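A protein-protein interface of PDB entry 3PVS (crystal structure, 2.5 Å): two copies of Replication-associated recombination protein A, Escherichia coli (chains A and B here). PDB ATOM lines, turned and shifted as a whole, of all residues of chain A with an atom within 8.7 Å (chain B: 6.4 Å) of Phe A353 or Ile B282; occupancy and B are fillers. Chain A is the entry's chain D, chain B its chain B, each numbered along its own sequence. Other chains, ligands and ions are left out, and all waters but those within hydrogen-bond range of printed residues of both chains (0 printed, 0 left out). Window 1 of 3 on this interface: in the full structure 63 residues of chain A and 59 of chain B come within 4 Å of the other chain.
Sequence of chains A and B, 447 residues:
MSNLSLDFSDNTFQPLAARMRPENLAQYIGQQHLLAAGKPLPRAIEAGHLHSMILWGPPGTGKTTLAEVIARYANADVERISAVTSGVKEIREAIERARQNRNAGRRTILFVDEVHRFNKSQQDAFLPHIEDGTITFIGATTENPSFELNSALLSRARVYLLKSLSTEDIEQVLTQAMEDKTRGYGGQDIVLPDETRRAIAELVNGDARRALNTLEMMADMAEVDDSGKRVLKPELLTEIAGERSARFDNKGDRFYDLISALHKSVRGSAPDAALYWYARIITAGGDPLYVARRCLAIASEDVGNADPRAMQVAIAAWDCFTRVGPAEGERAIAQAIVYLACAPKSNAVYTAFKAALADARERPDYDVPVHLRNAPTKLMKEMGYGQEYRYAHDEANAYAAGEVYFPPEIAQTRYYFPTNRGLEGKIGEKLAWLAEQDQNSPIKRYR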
ATOM      1  N   SER A 300      -6.187 -15.244   2.486  1.00  0.00           N
ATOM      2  CA  SER A 300      -5.252 -16.291   2.014  1.00  0.00           C
ATOM      3  C   SER A 300      -5.482 -17.682   2.598  1.00  0.00           C
ATOM      4  O   SER A 300      -5.130 -18.681   1.984  1.00  0.00           O
ATOM      5  CB  SER A 300      -3.767 -15.877   2.098  1.00  0.00           C
ATOM      6  OG  SER A 300      -3.216 -16.010   3.406  1.00  0.00           O
ATOM      7  N   ASN A 347      -9.180 -23.932   1.882  1.00  0.00           N
ATOM      8  CA  ASN A 347      -7.981 -23.843   2.690  1.00  0.00           C
ATOM      9  C   ASN A 347      -6.800 -24.547   2.056  1.00  0.00           C
ATOM     10  O   ASN A 347      -5.813 -24.781   2.738  1.00  0.00           O
ATOM     11  CB  ASN A 347      -8.202 -24.291   4.142  1.00  0.00           C
ATOM     12  CG  ASN A 347      -8.341 -25.793   4.301  1.00  0.00           C
ATOM     13  OD1 ASN A 347      -8.529 -26.542   3.343  1.00  0.00           O
ATOM     14  ND2 ASN A 347      -8.277 -26.231   5.541  1.00  0.00           N
ATOM     15  N   ALA A 348      -6.903 -24.836   0.743  1.00  0.00           N
ATOM     16  CA  ALA A 348      -5.898 -25.624   0.026  1.00  0.00           C
ATOM     17  C   ALA A 348      -4.515 -24.962  -0.132  1.00  0.00           C
ATOM     18  O   ALA A 348      -3.511 -25.673  -0.139  1.00  0.00           O
ATOM     19  CB  ALA A 348      -6.404 -26.065  -1.258  1.00  0.00           C
ATOM     20  N   VAL A 349      -4.433 -23.632  -0.214  1.00  0.00           N
ATOM     21  CA  VAL A 349      -3.139 -22.943  -0.250  1.00  0.00           C
ATOM     22  C   VAL A 349      -2.527 -22.984   1.153  1.00  0.00           C
ATOM     23  O   VAL A 349      -1.352 -23.291   1.334  1.00  0.00           O
ATOM     24  CB  VAL A 349      -3.299 -21.465  -0.734  1.00  0.00           C
ATOM     25  CG1 VAL A 349      -2.077 -20.565  -0.373  1.00  0.00           C
ATOM     26  CG2 VAL A 349      -3.583 -21.416  -2.233  1.00  0.00           C
ATOM     27  N   TYR A 350      -3.339 -22.659   2.144  1.00  0.00           N
ATOM     28  CA  TYR A 350      -2.962 -22.753   3.536  1.00  0.00           C
ATOM     29  C   TYR A 350      -2.401 -24.136   3.847  1.00  0.00           C
ATOM     30  O   TYR A 350      -1.281 -24.235   4.305  1.00  0.00           O
ATOM     31  CB  TYR A 350      -4.177 -22.431   4.415  1.00  0.00           C
ATOM     32  CG  TYR A 350      -3.953 -22.672   5.876  1.00  0.00           C
ATOM     33  CD1 TYR A 350      -3.202 -21.791   6.647  1.00  0.00           C
ATOM     34  CD2 TYR A 350      -4.485 -23.800   6.495  1.00  0.00           C
ATOM     35  CE1 TYR A 350      -2.985 -22.022   8.015  1.00  0.00           C
ATOM     36  CE2 TYR A 350      -4.279 -24.044   7.837  1.00  0.00           C
ATOM     37  CZ  TYR A 350      -3.530 -23.145   8.588  1.00  0.00           C
ATOM     38  OH  TYR A 350      -3.327 -23.423   9.916  1.00  0.00           O
ATOM     39  N   THR A 351      -3.158 -25.206   3.589  1.00  0.00           N
ATOM     40  CA  THR A 351      -2.646 -26.580   3.873  1.00  0.00           C
ATOM     41  C   THR A 351      -1.419 -26.891   3.025  1.00  0.00           C
ATOM     42  O   THR A 351      -0.486 -27.526   3.524  1.00  0.00           O
ATOM     43  CB  THR A 351      -3.702 -27.760   3.808  1.00  0.00           C
ATOM     44  OG1 THR A 351      -4.210 -27.944   2.481  1.00  0.00           O
ATOM     45  CG2 THR A 351      -4.879 -27.508   4.755  1.00  0.00           C
ATOM     46  N   ALA A 352      -1.382 -26.395   1.784  1.00  0.00           N
ATOM     47  CA  ALA A 352      -0.242 -26.736   0.926  1.00  0.00           C
ATOM     48  C   ALA A 352       1.043 -26.111   1.457  1.00  0.00           C
ATOM     49  O   ALA A 352       2.054 -26.796   1.572  1.00  0.00           O
ATOM     50  CB  ALA A 352      -0.481 -26.397  -0.578  1.00  0.00           C
ATOM     51  N   PHE A 353       0.970 -24.845   1.859  1.00  0.00           N
ATOM     52  CA  PHE A 353       2.130 -24.100   2.376  1.00  0.00           C
ATOM     53  C   PHE A 353       2.635 -24.614   3.742  1.00  0.00           C
ATOM     54  O   PHE A 353       3.834 -24.686   3.980  1.00  0.00           O
ATOM     55  CB  PHE A 353       1.817 -22.592   2.400  1.00  0.00           C
ATOM     56  CG  PHE A 353       2.965 -21.725   2.866  1.00  0.00           C
ATOM     57  CD1 PHE A 353       4.276 -21.966   2.420  1.00  0.00           C
ATOM     58  CD2 PHE A 353       2.737 -20.663   3.752  1.00  0.00           C
ATOM     59  CE1 PHE A 353       5.330 -21.179   2.870  1.00  0.00           C
ATOM     60  CE2 PHE A 353       3.753 -19.853   4.173  1.00  0.00           C
ATOM     61  CZ  PHE A 353       5.067 -20.101   3.739  1.00  0.00           C
ATOM     62  N   LYS A 354       1.719 -24.989   4.628  1.00  0.00           N
ATOM     63  CA  LYS A 354       2.046 -25.691   5.907  1.00  0.00           C
ATOM     64  C   LYS A 354       2.882 -26.978   5.676  1.00  0.00           C
ATOM     65  O   LYS A 354       3.909 -27.180   6.291  1.00  0.00           O
ATOM     66  CB  LYS A 354       0.731 -26.038   6.572  1.00  0.00           C
ATOM     67  CG  LYS A 354       0.723 -26.351   8.015  1.00  0.00           C
ATOM     68  CD  LYS A 354      -0.728 -26.696   8.329  1.00  0.00           C
ATOM     69  CE  LYS A 354      -1.044 -26.804   9.822  1.00  0.00           C
ATOM     70  NZ  LYS A 354      -2.097 -27.891  10.018  1.00  0.00           N
ATOM     71  N   ALA A 355       2.469 -27.816   4.731  1.00  0.00           N
ATOM     72  CA  ALA A 355       3.190 -29.057   4.416  1.00  0.00           C
ATOM     73  C   ALA A 355       4.610 -28.773   3.821  1.00  0.00           C
ATOM     74  O   ALA A 355       5.592 -29.472   4.132  1.00  0.00           O
ATOM     75  CB  ALA A 355       2.331 -29.932   3.476  1.00  0.00           C
ATOM     76  N   ALA A 356       4.715 -27.732   2.989  1.00  0.00           N
ATOM     77  CA  ALA A 356       6.003 -27.382   2.393  1.00  0.00           C
ATOM     78  C   ALA A 356       6.946 -26.900   3.446  1.00  0.00           C
ATOM     79  O   ALA A 356       8.123 -27.240   3.432  1.00  0.00           O
ATOM     80  CB  ALA A 356       5.841 -26.327   1.299  1.00  0.00           C
ATOM     81  N   LEU A 357       6.430 -26.090   4.366  1.00  0.00           N
ATOM     82  CA  LEU A 357       7.211 -25.641   5.484  1.00  0.00           C
ATOM     83  C   LEU A 357       7.732 -26.827   6.288  1.00  0.00           C
ATOM     84  O   LEU A 357       8.924 -26.896   6.603  1.00  0.00           O
ATOM     85  CB  LEU A 357       6.371 -24.734   6.372  1.00  0.00           C
ATOM     86  CG  LEU A 357       6.268 -23.256   5.959  1.00  0.00           C
ATOM     87  CD1 LEU A 357       5.266 -22.532   6.861  1.00  0.00           C
ATOM     88  CD2 LEU A 357       7.691 -22.539   5.899  1.00  0.00           C
ATOM     89  N   ALA A 358       6.835 -27.755   6.634  1.00  0.00           N
ATOM     90  CA  ALA A 358       7.225 -28.929   7.415  1.00  0.00           C
ATOM     91  C   ALA A 358       8.401 -29.659   6.711  1.00  0.00           C
ATOM     92  O   ALA A 358       9.461 -29.846   7.328  1.00  0.00           O
ATOM     93  CB  ALA A 358       6.017 -29.844   7.705  1.00  0.00           C
ATOM     94  N   ASP A 359       8.263 -29.984   5.422  1.00  0.00           N
ATOM     95  CA  ASP A 359       9.381 -30.579   4.661  1.00  0.00           C
ATOM     96  C   ASP A 359      10.677 -29.774   4.697  1.00  0.00           C
ATOM     97  O   ASP A 359      11.759 -30.333   4.791  1.00  0.00           O
ATOM     98  CB  ASP A 359       9.043 -30.693   3.183  1.00  0.00           C
ATOM     99  CG  ASP A 359       8.562 -32.056   2.785  1.00  0.00           C
ATOM    100  OD1 ASP A 359       8.656 -32.989   3.617  1.00  0.00           O
ATOM    101  OD2 ASP A 359       8.087 -32.188   1.622  1.00  0.00           O
ATOM    102  N   ALA A 360      10.603 -28.462   4.532  1.00  0.00           N
ATOM    103  CA  ALA A 360      11.828 -27.708   4.550  1.00  0.00           C
ATOM    104  C   ALA A 360      12.386 -27.659   5.960  1.00  0.00           C
ATOM    105  O   ALA A 360      13.571 -27.472   6.146  1.00  0.00           O
ATOM    106  CB  ALA A 360      11.614 -26.300   3.991  1.00  0.00           C
ATOM    107  N   ARG A 361      11.549 -27.812   6.968  1.00  0.00           N
ATOM    108  CA  ARG A 361      12.077 -27.788   8.324  1.00  0.00           C
ATOM    109  C   ARG A 361      12.567 -29.151   8.822  1.00  0.00           C
ATOM    110  O   ARG A 361      13.433 -29.209   9.659  1.00  0.00           O
ATOM    111  CB  ARG A 361      11.055 -27.237   9.303  1.00  0.00           C
ATOM    112  CG  ARG A 361      10.925 -25.763   9.248  1.00  0.00           C
ATOM    113  CD  ARG A 361       9.586 -25.325   9.808  1.00  0.00           C
ATOM    114  NE  ARG A 361       9.462 -23.871   9.684  1.00  0.00           N
ATOM    115  CZ  ARG A 361       8.340 -23.177   9.843  1.00  0.00           C
ATOM    116  NH1 ARG A 361       7.197 -23.786  10.157  1.00  0.00           N
ATOM    117  NH2 ARG A 361       8.381 -21.858   9.690  1.00  0.00           N
ATOM    118  N   TYR A 415       1.551 -31.227  -2.429  1.00  0.00           N
ATOM    119  CA  TYR A 415       1.142 -30.447  -1.313  1.00  0.00           C
ATOM    120  C   TYR A 415      -0.205 -29.854  -1.600  1.00  0.00           C
ATOM    121  O   TYR A 415      -0.990 -29.623  -0.671  1.00  0.00           O
ATOM    122  CB  TYR A 415       2.078 -29.273  -1.163  1.00  0.00           C
ATOM    123  CG  TYR A 415       3.498 -29.581  -0.823  1.00  0.00           C
ATOM    124  CD1 TYR A 415       3.832 -30.554   0.140  1.00  0.00           C
ATOM    125  CD2 TYR A 415       4.521 -28.850  -1.403  1.00  0.00           C
ATOM    126  CE1 TYR A 415       5.147 -30.779   0.481  1.00  0.00           C
ATOM    127  CE2 TYR A 415       5.833 -29.083  -1.090  1.00  0.00           C
ATOM    128  CZ  TYR A 415       6.149 -30.026  -0.145  1.00  0.00           C
ATOM    129  OH  TYR A 415       7.467 -30.213   0.160  1.00  0.00           O
ATOM    130  N   TYR A 416      -0.450 -29.545  -2.874  1.00  0.00           N
ATOM    131  CA  TYR A 416      -1.533 -28.678  -3.228  1.00  0.00           C
ATOM    132  C   TYR A 416      -2.646 -29.473  -3.867  1.00  0.00           C
ATOM    133  O   TYR A 416      -2.494 -29.987  -4.978  1.00  0.00           O
ATOM    134  CB  TYR A 416      -1.060 -27.557  -4.156  1.00  0.00           C
ATOM    135  CG  TYR A 416      -2.169 -26.627  -4.605  1.00  0.00           C
ATOM    136  CD1 TYR A 416      -2.940 -25.935  -3.677  1.00  0.00           C
ATOM    137  CD2 TYR A 416      -2.440 -26.425  -5.965  1.00  0.00           C
ATOM    138  CE1 TYR A 416      -3.949 -25.074  -4.087  1.00  0.00           C
ATOM    139  CE2 TYR A 416      -3.443 -25.555  -6.386  1.00  0.00           C
ATOM    140  CZ  TYR A 416      -4.196 -24.895  -5.423  1.00  0.00           C
ATOM    141  OH  TYR A 416      -5.215 -24.048  -5.791  1.00  0.00           O
ATOM    142  N   PHE A 417      -3.786 -29.526  -3.175  1.00  0.00           N
ATOM    143  CA  PHE A 417      -4.960 -30.228  -3.679  1.00  0.00           C
ATOM    144  C   PHE A 417      -6.131 -29.264  -3.842  1.00  0.00           C
ATOM    145  O   PHE A 417      -6.931 -29.081  -2.915  1.00  0.00           O
ATOM    146  CB  PHE A 417      -5.313 -31.396  -2.753  1.00  0.00           C
ATOM    147  CG  PHE A 417      -4.203 -32.428  -2.649  1.00  0.00           C
ATOM    148  CD1 PHE A 417      -4.187 -33.537  -3.506  1.00  0.00           C
ATOM    149  CD2 PHE A 417      -3.139 -32.248  -1.724  1.00  0.00           C
ATOM    150  CE1 PHE A 417      -3.150 -34.493  -3.410  1.00  0.00           C
ATOM    151  CE2 PHE A 417      -2.121 -33.160  -1.621  1.00  0.00           C
ATOM    152  CZ  PHE A 417      -2.109 -34.294  -2.467  1.00  0.00           C
ATOM    153  N   LEU B 275       6.356 -24.174  -3.930  1.00  0.00           N
ATOM    154  CA  LEU B 275       6.201 -23.974  -2.485  1.00  0.00           C
ATOM    155  C   LEU B 275       7.380 -24.597  -1.730  1.00  0.00           C
ATOM    156  O   LEU B 275       7.852 -24.013  -0.721  1.00  0.00           O
ATOM    157  CB  LEU B 275       4.927 -24.615  -1.988  1.00  0.00           C
ATOM    158  CG  LEU B 275       3.648 -23.895  -2.351  1.00  0.00           C
ATOM    159  CD1 LEU B 275       2.500 -24.801  -2.033  1.00  0.00           C
ATOM    160  CD2 LEU B 275       3.509 -22.535  -1.603  1.00  0.00           C
ATOM    161  N   TRP B 277      10.603 -24.861  -2.725  1.00  0.00           N
ATOM    162  CA  TRP B 277      11.812 -24.021  -2.774  1.00  0.00           C
ATOM    163  C   TRP B 277      11.609 -22.717  -1.986  1.00  0.00           C
ATOM    164  O   TRP B 277      12.503 -22.228  -1.312  1.00  0.00           O
ATOM    165  CB  TRP B 277      12.235 -23.749  -4.221  1.00  0.00           C
ATOM    166  CG  TRP B 277      12.604 -24.974  -4.931  1.00  0.00           C
ATOM    167  CD1 TRP B 277      12.015 -25.475  -6.040  1.00  0.00           C
ATOM    168  CD2 TRP B 277      13.657 -25.868  -4.598  1.00  0.00           C
ATOM    169  NE1 TRP B 277      12.623 -26.631  -6.426  1.00  0.00           N
ATOM    170  CE2 TRP B 277      13.636 -26.899  -5.541  1.00  0.00           C
ATOM    171  CE3 TRP B 277      14.627 -25.882  -3.599  1.00  0.00           C
ATOM    172  CZ2 TRP B 277      14.549 -27.975  -5.507  1.00  0.00           C
ATOM    173  CZ3 TRP B 277      15.533 -26.942  -3.544  1.00  0.00           C
ATOM    174  CH2 TRP B 277      15.500 -27.970  -4.504  1.00  0.00           C
ATOM    175  N   TYR B 278      10.399 -22.189  -2.066  1.00  0.00           N
ATOM    176  CA  TYR B 278      10.025 -20.995  -1.311  1.00  0.00           C
ATOM    177  C   TYR B 278      10.218 -21.267   0.156  1.00  0.00           C
ATOM    178  O   TYR B 278      10.859 -20.474   0.862  1.00  0.00           O
ATOM    179  CB  TYR B 278       8.564 -20.621  -1.591  1.00  0.00           C
ATOM    180  CG  TYR B 278       8.075 -19.460  -0.787  1.00  0.00           C
ATOM    181  CD1 TYR B 278       8.862 -18.284  -0.619  1.00  0.00           C
ATOM    182  CD2 TYR B 278       6.822 -19.498  -0.214  1.00  0.00           C
ATOM    183  CE1 TYR B 278       8.393 -17.197   0.122  1.00  0.00           C
ATOM    184  CE2 TYR B 278       6.353 -18.423   0.527  1.00  0.00           C
ATOM    185  CZ  TYR B 278       7.143 -17.282   0.685  1.00  0.00           C
ATOM    186  OH  TYR B 278       6.615 -16.272   1.430  1.00  0.00           O
ATOM    187  N   ALA B 279       9.690 -22.397   0.622  1.00  0.00           N
ATOM    188  CA  ALA B 279       9.815 -22.764   2.015  1.00  0.00           C
ATOM    189  C   ALA B 279      11.267 -22.935   2.382  1.00  0.00           C
ATOM    190  O   ALA B 279      11.667 -22.577   3.475  1.00  0.00           O
ATOM    191  CB  ALA B 279       9.046 -24.025   2.291  1.00  0.00           C
ATOM    192  N   ARG B 280      12.080 -23.474   1.472  1.00  0.00           N
ATOM    193  CA  ARG B 280      13.517 -23.627   1.777  1.00  0.00           C
ATOM    194  C   ARG B 280      14.192 -22.261   1.937  1.00  0.00           C
ATOM    195  O   ARG B 280      15.053 -22.106   2.787  1.00  0.00           O
ATOM    196  CB  ARG B 280      14.265 -24.504   0.748  1.00  0.00           C
ATOM    197  CG  ARG B 280      14.012 -26.035   0.836  1.00  0.00           C
ATOM    198  CD  ARG B 280      14.795 -26.764   1.987  1.00  0.00           C
ATOM    199  NE  ARG B 280      16.196 -26.489   1.815  1.00  0.00           N
ATOM    200  CZ  ARG B 280      16.978 -27.067   0.912  1.00  0.00           C
ATOM    201  NH1 ARG B 280      16.521 -28.071   0.141  1.00  0.00           N
ATOM    202  NH2 ARG B 280      18.246 -26.657   0.815  1.00  0.00           N
ATOM    203  N   ILE B 281      13.778 -21.265   1.155  1.00  0.00           N
ATOM    204  CA  ILE B 281      14.346 -19.911   1.252  1.00  0.00           C
ATOM    205  C   ILE B 281      14.003 -19.197   2.578  1.00  0.00           C
ATOM    206  O   ILE B 281      14.889 -18.735   3.301  1.00  0.00           O
ATOM    207  CB  ILE B 281      13.915 -19.078   0.050  1.00  0.00           C
ATOM    208  CG1 ILE B 281      14.423 -19.735  -1.243  1.00  0.00           C
ATOM    209  CG2 ILE B 281      14.392 -17.620   0.198  1.00  0.00           C
ATOM    210  CD1 ILE B 281      13.633 -19.339  -2.492  1.00  0.00           C
ATOM    211  N   ILE B 282      12.716 -19.104   2.883  1.00  0.00           N
ATOM    212  CA  ILE B 282      12.207 -18.561   4.147  1.00  0.00           C
ATOM    213  C   ILE B 282      12.952 -19.144   5.348  1.00  0.00           C
ATOM    214  O   ILE B 282      13.495 -18.425   6.190  1.00  0.00           O
ATOM    215  CB  ILE B 282      10.743 -19.019   4.371  1.00  0.00           C
ATOM    216  CG1 ILE B 282       9.784 -18.360   3.409  1.00  0.00           C
ATOM    217  CG2 ILE B 282      10.272 -18.702   5.798  1.00  0.00           C
ATOM    218  CD1 ILE B 282       8.348 -18.804   3.693  1.00  0.00           C
ATOM    219  N   THR B 283      12.950 -20.469   5.437  1.00  0.00           N
ATOM    220  CA  THR B 283      13.500 -21.101   6.615  1.00  0.00           C
ATOM    221  C   THR B 283      15.032 -21.057   6.676  1.00  0.00           C
ATOM    222  O   THR B 283      15.582 -21.092   7.771  1.00  0.00           O
ATOM    223  CB  THR B 283      12.935 -22.538   6.867  1.00  0.00           C
ATOM    224  OG1 THR B 283      13.588 -23.474   6.024  1.00  0.00           O
ATOM    225  CG2 THR B 283      11.408 -22.590   6.632  1.00  0.00           C
ATOM    226  N   ALA B 284      15.734 -20.944   5.550  1.00  0.00           N
ATOM    227  CA  ALA B 284      17.170 -20.647   5.639  1.00  0.00           C
ATOM    228  C   ALA B 284      17.444 -19.159   5.931  1.00  0.00           C
ATOM    229  O   ALA B 284      18.586 -18.730   5.841  1.00  0.00           O
ATOM    230  CB  ALA B 284      17.904 -21.096   4.395  1.00  0.00           C
ATOM    231  N   GLY B 285      16.405 -18.377   6.248  1.00  0.00           N
ATOM    232  CA  GLY B 285      16.522 -16.922   6.585  1.00  0.00           C
ATOM    233  C   GLY B 285      16.493 -15.909   5.424  1.00  0.00           C
ATOM    234  O   GLY B 285      16.892 -14.733   5.577  1.00  0.00           O
ATOM    235  N   GLY B 286      16.036 -16.350   4.250  1.00  0.00           N
ATOM    236  CA  GLY B 286      15.947 -15.458   3.104  1.00  0.00           C
ATOM    237  C   GLY B 286      14.804 -14.478   3.298  1.00  0.00           C
ATOM    238  O   GLY B 286      13.806 -14.790   3.940  1.00  0.00           O
ATOM    239  N   ASP B 287      14.960 -13.286   2.741  1.00  0.00           N
ATOM    240  CA  ASP B 287      13.975 -12.222   2.839  1.00  0.00           C
ATOM    241  C   ASP B 287      12.779 -12.495   1.918  1.00  0.00           C
ATOM    242  O   ASP B 287      12.920 -12.561   0.707  1.00  0.00           O
ATOM    243  CB  ASP B 287      14.656 -10.935   2.428  1.00  0.00           C
ATOM    244  CG  ASP B 287      13.814  -9.714   2.652  1.00  0.00           C
ATOM    245  OD1 ASP B 287      12.592  -9.807   2.928  1.00  0.00           O
ATOM    246  OD2 ASP B 287      14.397  -8.620   2.517  1.00  0.00           O
ATOM    247  N   PRO B 288      11.584 -12.629   2.495  1.00  0.00           N
ATOM    248  CA  PRO B 288      10.445 -12.984   1.654  1.00  0.00           C
ATOM    249  C   PRO B 288      10.116 -11.924   0.584  1.00  0.00           C
ATOM    250  O   PRO B 288       9.561 -12.285  -0.462  1.00  0.00           O
ATOM    251  CB  PRO B 288       9.296 -13.152   2.660  1.00  0.00           C
ATOM    252  CG  PRO B 288       9.960 -13.152   4.023  1.00  0.00           C
ATOM    253  CD  PRO B 288      11.204 -12.390   3.890  1.00  0.00           C
ATOM    254  N   VAL B 291      11.706 -12.600  -2.524  1.00  0.00           N
ATOM    255  CA  VAL B 291      10.845 -13.499  -3.286  1.00  0.00           C
ATOM    256  C   VAL B 291       9.672 -12.753  -3.940  1.00  0.00           C
ATOM    257  O   VAL B 291       9.341 -13.025  -5.108  1.00  0.00           O
ATOM    258  CB  VAL B 291      10.352 -14.673  -2.434  1.00  0.00           C
ATOM    259  CG1 VAL B 291       9.385 -15.573  -3.215  1.00  0.00           C
ATOM    260  CG2 VAL B 291      11.546 -15.475  -1.891  1.00  0.00           C
ATOM    261  N   ALA B 327       4.356 -13.197   9.780  1.00  0.00           N
ATOM    262  CA  ALA B 327       3.497 -14.336  10.153  1.00  0.00           C
ATOM    263  C   ALA B 327       2.623 -14.816   8.976  1.00  0.00           C
ATOM    264  O   ALA B 327       2.720 -15.966   8.556  1.00  0.00           O
ATOM    265  CB  ALA B 327       2.610 -14.018  11.400  1.00  0.00           C
ATOM    266  N   GLU B 330       3.946 -14.135   4.542  1.00  0.00           N
ATOM    267  CA  GLU B 330       4.579 -15.272   3.861  1.00  0.00           C
ATOM    268  C   GLU B 330       3.587 -16.140   3.170  1.00  0.00           C
ATOM    269  O   GLU B 330       3.822 -16.549   2.013  1.00  0.00           O
ATOM    270  CB  GLU B 330       5.412 -16.089   4.817  1.00  0.00           C
ATOM    271  CG  GLU B 330       6.669 -15.339   5.218  1.00  0.00           C
ATOM    272  CD  GLU B 330       7.459 -15.976   6.338  1.00  0.00           C
ATOM    273  OE1 GLU B 330       7.107 -17.079   6.817  1.00  0.00           O
ATOM    274  OE2 GLU B 330       8.454 -15.349   6.727  1.00  0.00           O
ATOM    275  N   ARG B 331       2.465 -16.387   3.839  1.00  0.00           N
ATOM    276  CA  ARG B 331       1.389 -17.147   3.223  1.00  0.00           C
ATOM    277  C   ARG B 331       0.786 -16.437   1.977  1.00  0.00           C
ATOM    278  O   ARG B 331       0.438 -17.091   0.996  1.00  0.00           O
ATOM    279  CB  ARG B 331       0.269 -17.504   4.208  1.00  0.00           C
ATOM    280  CG  ARG B 331      -0.681 -18.489   3.532  1.00  0.00           C
ATOM    281  CD  ARG B 331      -1.929 -18.875   4.261  1.00  0.00           C
ATOM    282  NE  ARG B 331      -2.543 -17.778   4.963  1.00  0.00           N
ATOM    283  CZ  ARG B 331      -2.399 -17.584   6.270  1.00  0.00           C
ATOM    284  NH1 ARG B 331      -3.018 -16.551   6.848  1.00  0.00           N
ATOM    285  NH2 ARG B 331      -1.639 -18.425   6.990  1.00  0.00           N
ATOM    286  N   ALA B 332       0.639 -15.121   2.037  1.00  0.00           N
ATOM    287  CA  ALA B 332       0.140 -14.395   0.912  1.00  0.00           C
ATOM    288  C   ALA B 332       1.113 -14.479  -0.283  1.00  0.00           C
ATOM    289  O   ALA B 332       0.639 -14.598  -1.420  1.00  0.00           O
ATOM    290  CB  ALA B 332      -0.155 -12.933   1.288  1.00  0.00           C
ATOM    291  N   ALA B 334       3.135 -17.058  -0.770  1.00  0.00           N
ATOM    292  CA  ALA B 334       2.880 -18.422  -1.216  1.00  0.00           C
ATOM    293  C   ALA B 334       1.614 -18.554  -2.066  1.00  0.00           C
ATOM    294  O   ALA B 334       1.571 -19.405  -2.959  1.00  0.00           O
ATOM    295  CB  ALA B 334       2.801 -19.365  -0.043  1.00  0.00           C
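The guanidinium group (NE) of Arg B331 is in hydrogen-bond range of the side-chain hydroxyl (OG) of Ser A300 (2.5 Å).
The side-chain hydroxyl (OH) of Tyr B278 sits at hydrogen-bond distance from the backbone carbonyl oxygen (O) of Glu B330 (2.9 Å).
O of Ala B279 sits close to OG1 of Thr B283 (3.3 Å).
Phe A353 touches just these residues of chain B: Tyr B278 (3.8 Å), Ile B282 (3.5 Å), Glu B330 (3.8 Å), Arg B331 (3.7 Å) and Ala B334 (3.7 Å).
Ile B282 touches just one residue of chain A: Phe A353.
Printed residues of chain A within 4 Å of Thr B283: Leu A357, Ala A360 and Arg A361.
Of the printed residues of chain B, Ala A352 touches Leu B275.
Of the printed residues of chain A, Ala B334 touches Phe A353 (3.7 Å).
Printed residues of chain B within 4 Å of Arg A361: Thr B283 (3.8 Å).
Ala A358 touches none of the printed residues of chain B.
Hydrophobic or aromatic side chains of chain B within 4 Å of the printed part of chain A: Leu B275, Tyr B278, Ala B279, Ile B282 and Ala B334.
Of the 19 printed residues of chain A, 8 touch a printed residue of chain B.
Hydrophobic or aromatic side chains of chain A within 4 Å of the printed part of chain B: Tyr A350, Ala A352, Phe A353, Ala A356, Leu A357 and Ala A360.
Among the printed residues, 16 pairs touch across the chains.
Among the printed residues, no Asp or Glu carboxylate lies within 4 Å of a Lys or Arg side-chain nitrogen of the other chain.
Ala A352 touches Leu B275 (CB to CD1, 3.7 Å).
Phe A353 touches Tyr B278.
C of Glu B330 touches CE2 of Phe A353, at 3.8 Å.
CE2 of Phe A353 touches N of Arg B331 (3.7 Å).
Ala B334 touches Phe A353 (CB to CG, 3.7 Å).
Ala A356 touches Ala B279.
Leu A357 touches Ala B279 (N to CB, 3.9 Å).
CD2 of Leu A357 touches CG2 of Thr B283 (3.8 Å).
CB of Ala A360 touches CD of Arg B280, at 3.8 Å.
Ala A360 touches Thr B283 (O to OG1, 3.9999 Å).
No position is printed for both chains.
Of the 16 pairs that touch across the chains among the printed residues, none has its exchanged pair printed and touching as well.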
